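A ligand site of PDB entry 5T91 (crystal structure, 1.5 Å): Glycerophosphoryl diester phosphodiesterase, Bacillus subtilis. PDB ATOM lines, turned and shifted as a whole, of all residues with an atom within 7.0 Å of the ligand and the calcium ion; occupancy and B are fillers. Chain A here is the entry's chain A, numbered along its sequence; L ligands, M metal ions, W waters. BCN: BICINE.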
ATOM      1  N   VAL A  16       3.767  29.057  22.016  1.00  0.00           N
ATOM      2  CA  VAL A  16       3.402  28.184  20.898  1.00  0.00           C
ATOM      3  C   VAL A  16       3.148  29.038  19.674  1.00  0.00           C
ATOM      4  O   VAL A  16       2.200  29.829  19.635  1.00  0.00           O
ATOM      5  CB  VAL A  16       2.164  27.327  21.205  1.00  0.00           C
ATOM      6  CG1 VAL A  16       1.930  26.282  20.076  1.00  0.00           C
ATOM      7  CG2 VAL A  16       2.318  26.628  22.549  1.00  0.00           C
ATOM      8  N   HIS A  18       1.641  29.668  16.589  1.00  0.00           N
ATOM      9  CA  HIS A  18       0.430  29.203  15.941  1.00  0.00           C
ATOM     10  C   HIS A  18       0.555  29.205  14.429  1.00  0.00           C
ATOM     11  O   HIS A  18       0.634  30.256  13.801  1.00  0.00           O
ATOM     12  CB  HIS A  18      -0.725  30.109  16.381  1.00  0.00           C
ATOM     13  CG  HIS A  18      -2.082  29.537  16.104  1.00  0.00           C
ATOM     14  ND1 HIS A  18      -3.008  30.174  15.310  1.00  0.00           N
ATOM     15  CD2 HIS A  18      -2.674  28.408  16.542  1.00  0.00           C
ATOM     16  CE1 HIS A  18      -4.115  29.452  15.251  1.00  0.00           C
ATOM     17  NE2 HIS A  18      -3.934  28.370  15.991  1.00  0.00           N
ATOM     18  N   ARG A  19       0.581  28.013  13.833  1.00  0.00           N
ATOM     19  CA  ARG A  19       0.892  27.858  12.405  1.00  0.00           C
ATOM     20  C   ARG A  19       2.248  28.477  12.059  1.00  0.00           C
ATOM     21  O   ARG A  19       2.465  28.906  10.926  1.00  0.00           O
ATOM     22  CB  ARG A  19      -0.221  28.444  11.543  1.00  0.00           C
ATOM     23  CG  ARG A  19      -1.606  28.211  12.121  1.00  0.00           C
ATOM     24  CD  ARG A  19      -2.748  28.532  11.177  1.00  0.00           C
ATOM     25  NE  ARG A  19      -3.994  28.416  11.910  1.00  0.00           N
ATOM     26  CZ  ARG A  19      -5.133  29.026  11.587  1.00  0.00           C
ATOM     27  NH1 ARG A  19      -5.224  29.792  10.506  1.00  0.00           N
ATOM     28  NH2 ARG A  19      -6.201  28.873  12.360  1.00  0.00           N
ATOM     29  N   HIS A  28       1.623  27.729   8.191  1.00  0.00           N
ATOM     30  CA  HIS A  28       1.873  26.305   7.884  1.00  0.00           C
ATOM     31  C   HIS A  28       2.746  26.127   6.655  1.00  0.00           C
ATOM     32  O   HIS A  28       2.455  25.291   5.773  1.00  0.00           O
ATOM     33  CB  HIS A  28       0.544  25.561   7.713  1.00  0.00           C
ATOM     34  CG  HIS A  28      -0.236  25.361   8.980  1.00  0.00           C
ATOM     35  ND1 HIS A  28       0.370  25.141  10.208  1.00  0.00           N
ATOM     36  CD2 HIS A  28      -1.572  25.335   9.213  1.00  0.00           C
ATOM     37  CE1 HIS A  28      -0.566  24.971  11.133  1.00  0.00           C
ATOM     38  NE2 HIS A  28      -1.744  25.088  10.555  1.00  0.00           N
ATOM     39  N   GLU A  45       3.412  24.918  15.676  1.00  0.00           N
ATOM     40  CA  GLU A  45       2.076  24.320  15.732  1.00  0.00           C
ATOM     41  C   GLU A  45       1.597  23.885  14.338  1.00  0.00           C
ATOM     42  O   GLU A  45       1.674  24.639  13.380  1.00  0.00           O
ATOM     43  CB  GLU A  45       1.085  25.315  16.387  1.00  0.00           C
ATOM     44  CG  GLU A  45      -0.269  24.718  16.710  1.00  0.00           C
ATOM     45  CD  GLU A  45      -1.369  25.124  15.738  1.00  0.00           C
ATOM     46  OE1 GLU A  45      -1.106  25.821  14.729  1.00  0.00           O
ATOM     47  OE2 GLU A  45      -2.529  24.735  16.017  1.00  0.00           O
ATOM     48  N   LEU A  46       1.123  22.633  14.248  1.00  0.00           N
ATOM     49  CA  LEU A  46       0.720  22.008  12.983  1.00  0.00           C
ATOM     50  C   LEU A  46      -0.743  21.528  13.024  1.00  0.00           C
ATOM     51  O   LEU A  46      -1.202  21.028  14.050  1.00  0.00           O
ATOM     52  CB  LEU A  46       1.619  20.798  12.658  1.00  0.00           C
ATOM     53  CG  LEU A  46       3.057  20.950  12.187  1.00  0.00           C
ATOM     54  CD1 LEU A  46       3.938  21.668  13.217  1.00  0.00           C
ATOM     55  CD2 LEU A  46       3.646  19.568  11.860  1.00  0.00           C
ATOM     56  N   ASP A  47      -1.441  21.659  11.892  1.00  0.00           N
ATOM     57  CA  ASP A  47      -2.751  21.045  11.663  1.00  0.00           C
ATOM     58  C   ASP A  47      -2.586  20.030  10.550  1.00  0.00           C
ATOM     59  O   ASP A  47      -1.868  20.312   9.607  1.00  0.00           O
ATOM     60  CB  ASP A  47      -3.807  22.065  11.226  1.00  0.00           C
ATOM     61  CG  ASP A  47      -4.107  23.102  12.293  1.00  0.00           C
ATOM     62  OD1 ASP A  47      -4.367  22.711  13.455  1.00  0.00           O
ATOM     63  OD2 ASP A  47      -4.108  24.313  11.964  1.00  0.00           O
ATOM     64  N   HIS A  60      -4.577  24.032   7.674  1.00  0.00           N
ATOM     65  CA  HIS A  60      -5.585  24.244   8.693  1.00  0.00           C
ATOM     66  C   HIS A  60      -6.989  23.840   8.247  1.00  0.00           C
ATOM     67  O   HIS A  60      -7.724  23.196   9.013  1.00  0.00           O
ATOM     68  CB  HIS A  60      -5.615  25.707   9.122  1.00  0.00           C
ATOM     69  CG  HIS A  60      -6.683  26.004  10.116  1.00  0.00           C
ATOM     70  ND1 HIS A  60      -6.633  25.564  11.414  1.00  0.00           N
ATOM     71  CD2 HIS A  60      -7.861  26.663   9.983  1.00  0.00           C
ATOM     72  CE1 HIS A  60      -7.715  25.953  12.059  1.00  0.00           C
ATOM     73  NE2 HIS A  60      -8.480  26.627  11.219  1.00  0.00           N
ATOM     74  N   TYR A 125       3.619  20.955  18.202  1.00  0.00           N
ATOM     75  CA  TYR A 125       2.287  20.959  18.787  1.00  0.00           C
ATOM     76  C   TYR A 125       1.333  20.568  17.668  1.00  0.00           C
ATOM     77  O   TYR A 125       1.031  21.397  16.806  1.00  0.00           O
ATOM     78  CB  TYR A 125       1.945  22.349  19.305  1.00  0.00           C
ATOM     79  CG  TYR A 125       1.184  22.424  20.605  1.00  0.00           C
ATOM     80  CD1 TYR A 125       1.720  23.073  21.712  1.00  0.00           C
ATOM     81  CD2 TYR A 125      -0.071  21.849  20.743  1.00  0.00           C
ATOM     82  CE1 TYR A 125       1.010  23.170  22.908  1.00  0.00           C
ATOM     83  CE2 TYR A 125      -0.777  21.916  21.935  1.00  0.00           C
ATOM     84  CZ  TYR A 125      -0.239  22.596  23.022  1.00  0.00           C
ATOM     85  OH  TYR A 125      -0.950  22.680  24.200  1.00  0.00           O
ATOM     86  N   GLU A 127      -2.145  18.944  15.804  1.00  0.00           N
ATOM     87  CA  GLU A 127      -3.575  18.665  15.943  1.00  0.00           C
ATOM     88  C   GLU A 127      -3.959  17.323  15.324  1.00  0.00           C
ATOM     89  O   GLU A 127      -3.451  16.950  14.287  1.00  0.00           O
ATOM     90  CB  GLU A 127      -4.440  19.754  15.309  1.00  0.00           C
ATOM     91  CG  GLU A 127      -5.892  19.659  15.753  1.00  0.00           C
ATOM     92  CD  GLU A 127      -6.896  19.922  14.657  1.00  0.00           C
ATOM     93  OE1 GLU A 127      -6.581  19.691  13.475  1.00  0.00           O
ATOM     94  OE2 GLU A 127      -8.027  20.342  14.978  1.00  0.00           O
ATOM     95  N   THR A 128      -4.864  16.626  16.007  1.00  0.00           N
ATOM     96  CA  THR A 128      -5.557  15.489  15.413  1.00  0.00           C
ATOM     97  C   THR A 128      -7.049  15.802  15.311  1.00  0.00           C
ATOM     98  O   THR A 128      -7.567  16.698  15.983  1.00  0.00           O
ATOM     99  CB  THR A 128      -5.375  14.189  16.233  1.00  0.00           C
ATOM    100  OG1 THR A 128      -5.771  14.406  17.587  1.00  0.00           O
ATOM    101  CG2 THR A 128      -3.927  13.713  16.203  1.00  0.00           C
ATOM    102  N   LYS A 129      -7.743  15.027  14.480  1.00  0.00           N
ATOM    103  CA  LYS A 129      -9.179  15.186  14.247  1.00  0.00           C
ATOM    104  C   LYS A 129      -9.913  14.060  14.947  1.00  0.00           C
ATOM    105  O   LYS A 129      -9.284  13.119  15.438  1.00  0.00           O
ATOM    106  CB  LYS A 129      -9.489  15.152  12.748  1.00  0.00           C
ATOM    107  CG  LYS A 129      -8.667  16.102  11.898  1.00  0.00           C
ATOM    108  CD  LYS A 129      -9.085  17.528  12.123  1.00  0.00           C
ATOM    109  CE  LYS A 129      -8.568  18.441  11.016  1.00  0.00           C
ATOM    110  NZ  LYS A 129      -9.077  19.828  11.212  1.00  0.00           N
ATOM    111  N   GLN A 163      -2.707  18.045  20.255  1.00  0.00           N
ATOM    112  CA  GLN A 163      -3.885  18.824  20.608  1.00  0.00           C
ATOM    113  C   GLN A 163      -5.076  18.338  19.821  1.00  0.00           C
ATOM    114  O   GLN A 163      -4.925  17.897  18.672  1.00  0.00           O
ATOM    115  CB  GLN A 163      -3.662  20.324  20.323  1.00  0.00           C
ATOM    116  CG  GLN A 163      -3.336  20.562  18.847  1.00  0.00           C
ATOM    117  CD  GLN A 163      -3.287  22.013  18.447  1.00  0.00           C
ATOM    118  OE1 GLN A 163      -3.843  22.894  19.121  1.00  0.00           O
ATOM    119  NE2 GLN A 163      -2.600  22.298  17.333  1.00  0.00           N
ATOM    120  N   SER A 164      -6.259  18.391  20.425  1.00  0.00           N
ATOM    121  CA  SER A 164      -7.460  18.090  19.647  1.00  0.00           C
ATOM    122  C   SER A 164      -8.743  18.579  20.298  1.00  0.00           C
ATOM    123  O   SER A 164      -8.854  18.573  21.522  1.00  0.00           O
ATOM    124  CB  SER A 164      -7.565  16.572  19.396  1.00  0.00           C
ATOM    125  OG  SER A 164      -8.685  16.244  18.574  1.00  0.00           O
ATOM    126  N   PHE A 165      -9.713  18.986  19.486  1.00  0.00           N
ATOM    127  CA  PHE A 165     -11.074  19.193  19.992  1.00  0.00           C
ATOM    128  C   PHE A 165     -11.748  17.863  20.345  1.00  0.00           C
ATOM    129  O   PHE A 165     -12.643  17.799  21.196  1.00  0.00           O
ATOM    130  CB  PHE A 165     -11.944  19.944  18.976  1.00  0.00           C
ATOM    131  CG  PHE A 165     -11.579  21.392  18.801  1.00  0.00           C
ATOM    132  CD1 PHE A 165     -11.943  22.331  19.759  1.00  0.00           C
ATOM    133  CD2 PHE A 165     -10.907  21.815  17.675  1.00  0.00           C
ATOM    134  CE1 PHE A 165     -11.613  23.687  19.584  1.00  0.00           C
ATOM    135  CE2 PHE A 165     -10.585  23.143  17.489  1.00  0.00           C
ATOM    136  CZ  PHE A 165     -10.937  24.088  18.458  1.00  0.00           C
ATOM    137  N   LEU A 185      -8.516  20.684  23.461  1.00  0.00           N
ATOM    138  CA  LEU A 185      -8.946  21.982  22.940  1.00  0.00           C
ATOM    139  C   LEU A 185     -10.402  22.226  23.283  1.00  0.00           C
ATOM    140  O   LEU A 185     -11.229  21.308  23.221  1.00  0.00           O
ATOM    141  CB  LEU A 185      -8.737  22.036  21.430  1.00  0.00           C
ATOM    142  CG  LEU A 185      -7.283  21.963  20.942  1.00  0.00           C
ATOM    143  CD1 LEU A 185      -7.242  21.915  19.427  1.00  0.00           C
ATOM    144  CD2 LEU A 185      -6.478  23.156  21.465  1.00  0.00           C
ATOM    145  N   LEU A 186     -10.723  23.461  23.644  1.00  0.00           N
ATOM    146  CA  LEU A 186     -12.069  23.807  24.075  1.00  0.00           C
ATOM    147  C   LEU A 186     -12.585  25.057  23.361  1.00  0.00           C
ATOM    148  O   LEU A 186     -11.960  26.112  23.401  1.00  0.00           O
ATOM    149  CB  LEU A 186     -12.103  24.047  25.586  1.00  0.00           C
ATOM    150  CG  LEU A 186     -11.665  22.888  26.487  1.00  0.00           C
ATOM    151  CD1 LEU A 186     -11.462  23.388  27.902  1.00  0.00           C
ATOM    152  CD2 LEU A 186     -12.696  21.757  26.456  1.00  0.00           C
ATOM    153  N   GLY A 210      -6.752  23.767  26.263  1.00  0.00           N
ATOM    154  CA  GLY A 210      -6.514  24.850  25.328  1.00  0.00           C
ATOM    155  C   GLY A 210      -7.812  25.491  24.888  1.00  0.00           C
ATOM    156  O   GLY A 210      -8.357  25.132  23.851  1.00  0.00           O
ATOM    157  N   HIS A 232      -3.174  26.657  27.843  1.00  0.00           N
ATOM    158  CA  HIS A 232      -2.692  27.323  26.640  1.00  0.00           C
ATOM    159  C   HIS A 232      -3.850  27.838  25.801  1.00  0.00           C
ATOM    160  O   HIS A 232      -4.295  27.156  24.895  1.00  0.00           O
ATOM    161  CB  HIS A 232      -1.846  26.370  25.781  1.00  0.00           C
ATOM    162  CG  HIS A 232      -0.697  25.735  26.498  1.00  0.00           C
ATOM    163  ND1 HIS A 232      -0.087  24.583  26.046  1.00  0.00           N
ATOM    164  CD2 HIS A 232      -0.019  26.114  27.613  1.00  0.00           C
ATOM    165  CE1 HIS A 232       0.909  24.267  26.860  1.00  0.00           C
ATOM    166  NE2 HIS A 232       0.963  25.175  27.823  1.00  0.00           N
ATOM    167  N   PRO A 233      -4.351  29.049  26.107  1.00  0.00           N
ATOM    168  CA  PRO A 233      -5.440  29.594  25.287  1.00  0.00           C
ATOM    169  C   PRO A 233      -4.996  29.989  23.878  1.00  0.00           C
ATOM    170  O   PRO A 233      -3.818  30.269  23.645  1.00  0.00           O
ATOM    171  CB  PRO A 233      -5.891  30.826  26.087  1.00  0.00           C
ATOM    172  CG  PRO A 233      -4.749  31.176  26.936  1.00  0.00           C
ATOM    173  CD  PRO A 233      -4.004  29.923  27.241  1.00  0.00           C
ATOM    174  N   TYR A 234      -5.956  30.003  22.960  1.00  0.00           N
ATOM    175  CA  TYR A 234      -5.744  30.452  21.577  1.00  0.00           C
ATOM    176  C   TYR A 234      -6.814  31.484  21.251  1.00  0.00           C
ATOM    177  O   TYR A 234      -7.839  31.519  21.921  1.00  0.00           O
ATOM    178  CB  TYR A 234      -5.835  29.261  20.593  1.00  0.00           C
ATOM    179  CG  TYR A 234      -7.227  28.656  20.559  1.00  0.00           C
ATOM    180  CD1 TYR A 234      -8.201  29.162  19.704  1.00  0.00           C
ATOM    181  CD2 TYR A 234      -7.568  27.591  21.393  1.00  0.00           C
ATOM    182  CE1 TYR A 234      -9.489  28.626  19.687  1.00  0.00           C
ATOM    183  CE2 TYR A 234      -8.853  27.051  21.385  1.00  0.00           C
ATOM    184  CZ  TYR A 234      -9.802  27.575  20.521  1.00  0.00           C
ATOM    185  OH  TYR A 234     -11.081  27.050  20.506  1.00  0.00           O
ATOM    186  N   THR A 235      -6.588  32.333  20.244  1.00  0.00           N
ATOM    187  CA  THR A 235      -5.295  32.585  19.630  1.00  0.00           C
ATOM    188  C   THR A 235      -4.922  33.983  20.063  1.00  0.00           C
ATOM    189  O   THR A 235      -5.615  34.945  19.700  1.00  0.00           O
ATOM    190  CB  THR A 235      -5.352  32.492  18.096  1.00  0.00           C
ATOM    191  OG1 THR A 235      -5.740  31.169  17.713  1.00  0.00           O
ATOM    192  CG2 THR A 235      -3.987  32.798  17.478  1.00  0.00           C
ATOM    193  N   PHE A 254      -1.128  29.975  22.449  1.00  0.00           N
ATOM    194  CA  PHE A 254      -0.997  29.884  20.994  1.00  0.00           C
ATOM    195  C   PHE A 254      -1.051  31.298  20.444  1.00  0.00           C
ATOM    196  O   PHE A 254      -2.046  32.009  20.651  1.00  0.00           O
ATOM    197  CB  PHE A 254      -2.124  29.056  20.348  1.00  0.00           C
ATOM    198  CG  PHE A 254      -2.226  27.623  20.815  1.00  0.00           C
ATOM    199  CD1 PHE A 254      -2.941  27.279  21.954  1.00  0.00           C
ATOM    200  CD2 PHE A 254      -1.672  26.591  20.037  1.00  0.00           C
ATOM    201  CE1 PHE A 254      -3.074  25.949  22.341  1.00  0.00           C
ATOM    202  CE2 PHE A 254      -1.794  25.268  20.436  1.00  0.00           C
ATOM    203  CZ  PHE A 254      -2.489  24.950  21.594  1.00  0.00           C
HETATM  204  N1  BCN L   1      -6.844  25.808  16.999  1.00  0.00           N
HETATM  205  C1  BCN L   1      -7.613  27.016  16.872  1.00  0.00           C
HETATM  206  C2  BCN L   1      -7.363  27.618  15.506  1.00  0.00           C
HETATM  207  O21 BCN L   1      -6.411  27.224  14.824  1.00  0.00           O
HETATM  208  O22 BCN L   1      -8.123  28.526  15.056  1.00  0.00           O
HETATM  209  C3  BCN L   1      -6.670  25.526  18.408  1.00  0.00           C
HETATM  210  C4  BCN L   1      -5.329  26.096  18.891  1.00  0.00           C
HETATM  211  O4  BCN L   1      -4.288  25.577  18.117  1.00  0.00           O
HETATM  212  C5  BCN L   1      -7.532  24.694  16.336  1.00  0.00           C
HETATM  213  C6  BCN L   1      -6.512  23.596  15.875  1.00  0.00           C
HETATM  214  O6  BCN L   1      -5.446  24.158  15.089  1.00  0.00           O
HETATM  215 CA    CA M   1      -4.632  26.034  15.769  1.00  0.00          CA
HETATM  216  O   HOH W   1      -9.256  29.661  12.701  1.00  0.00           O
HETATM  217  O   HOH W   2      -3.637  26.197  13.661  1.00  0.00           O
HETATM  218  O   HOH W   3      -6.852  31.384  15.072  1.00  0.00           O
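OD1 of Asp 47 lies close to O6 of the ligand (2.4 Å).
An oxygen (O4) of the ligand lies close to the side-chain amide oxygen (OE1) of Gln 163, 2.9 Å away.
The guanidinium group (NH2) of Arg 19 is in salt-bridge range of an oxygen (O22) of the ligand (3.3 Å).
ND1 of His 60 sits at hydrogen-bond distance from OD2 of Asp 47.
OE2 of Glu 45 sits close to NE2 of Gln 163.
The backbone NH (N) of Arg 19 sits at hydrogen-bond distance from the side-chain carboxylate (OE1) of Glu 45 (2.9 Å).
ND1 of His 28 lies close to O of Glu 45 (3.5 Å).
The backbone NH (N) of Phe 254 sits at hydrogen-bond distance from the backbone carbonyl oxygen (O) of Pro 233 (3.0 Å).
The backbone carbonyl oxygen (O) of Leu 46 lies within hydrogen-bond range of the backbone NH (N) of Glu 127, 2.9 Å away.
The side-chain amino group (NZ) of Lys 129 is in salt-bridge range of the side-chain carboxylate (OE1) of Glu 127.
The backbone NH of Leu 185 lies within hydrogen-bond range of the backbone carbonyl oxygen of Ser 164.
His 60 touches the ligand.
Glu 127 touches the ligand (OE2 to C6, 3.7 Å).
Phe 165 touches the ligand.
CD1 of Leu 185 touches C3 of the ligand, 3.8 Å away.
Tyr 234 touches the ligand (CG to C4, 3.6 Å).
Phe 254 touches the ligand.
11 residues have an atom within 4 Å of the ligand: His 18, Arg 19, Glu 45, Asp 47, His 60, Glu 127, Gln 163, Phe 165, Leu 185, Tyr 234 and Phe 254.
The nearest printed residue that does not touch the ligand is Thr 235 (4.4 Å).
Within 4 Å of the calcium ion: His 18 and Glu 45.
The nearest printed residue that does not touch the calcium ion is Asp 47 (4.1 Å).
The calcium ion is bound by an oxygen (O6) of the ligand (2.2 Å), water W2 (2.3 Å), an oxygen (O21) of the ligand (2.3 Å), an oxygen (O4) of the ligand (2.4 Å), a ring nitrogen (NE2) of His 18 (2.4 Å), the side-chain carboxylate (OE2) of Glu 45 (2.5 Å) and a nitrogen (N1) of the ligand (2.5 Å).
The calcium ion has seven donor atoms within binding distance.
Water W2 lies within hydrogen-bond range of the side-chain carboxylate of Asp 47 (2.6 Å), the side-chain carboxylate of Glu 45 (2.8 Å) and the guanidinium group of Arg 19 (2.8 Å).
Water W1 lies within hydrogen-bond range of O22 of the ligand (2.8 Å), NH2 of Arg 19 (3.2 Å) and NE2 of His 60 (3.5 Å).
Water W3 lies within hydrogen-bond range of OG1 of Thr 235 (2.9 Å) and O22 of the ligand (3.1 Å).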
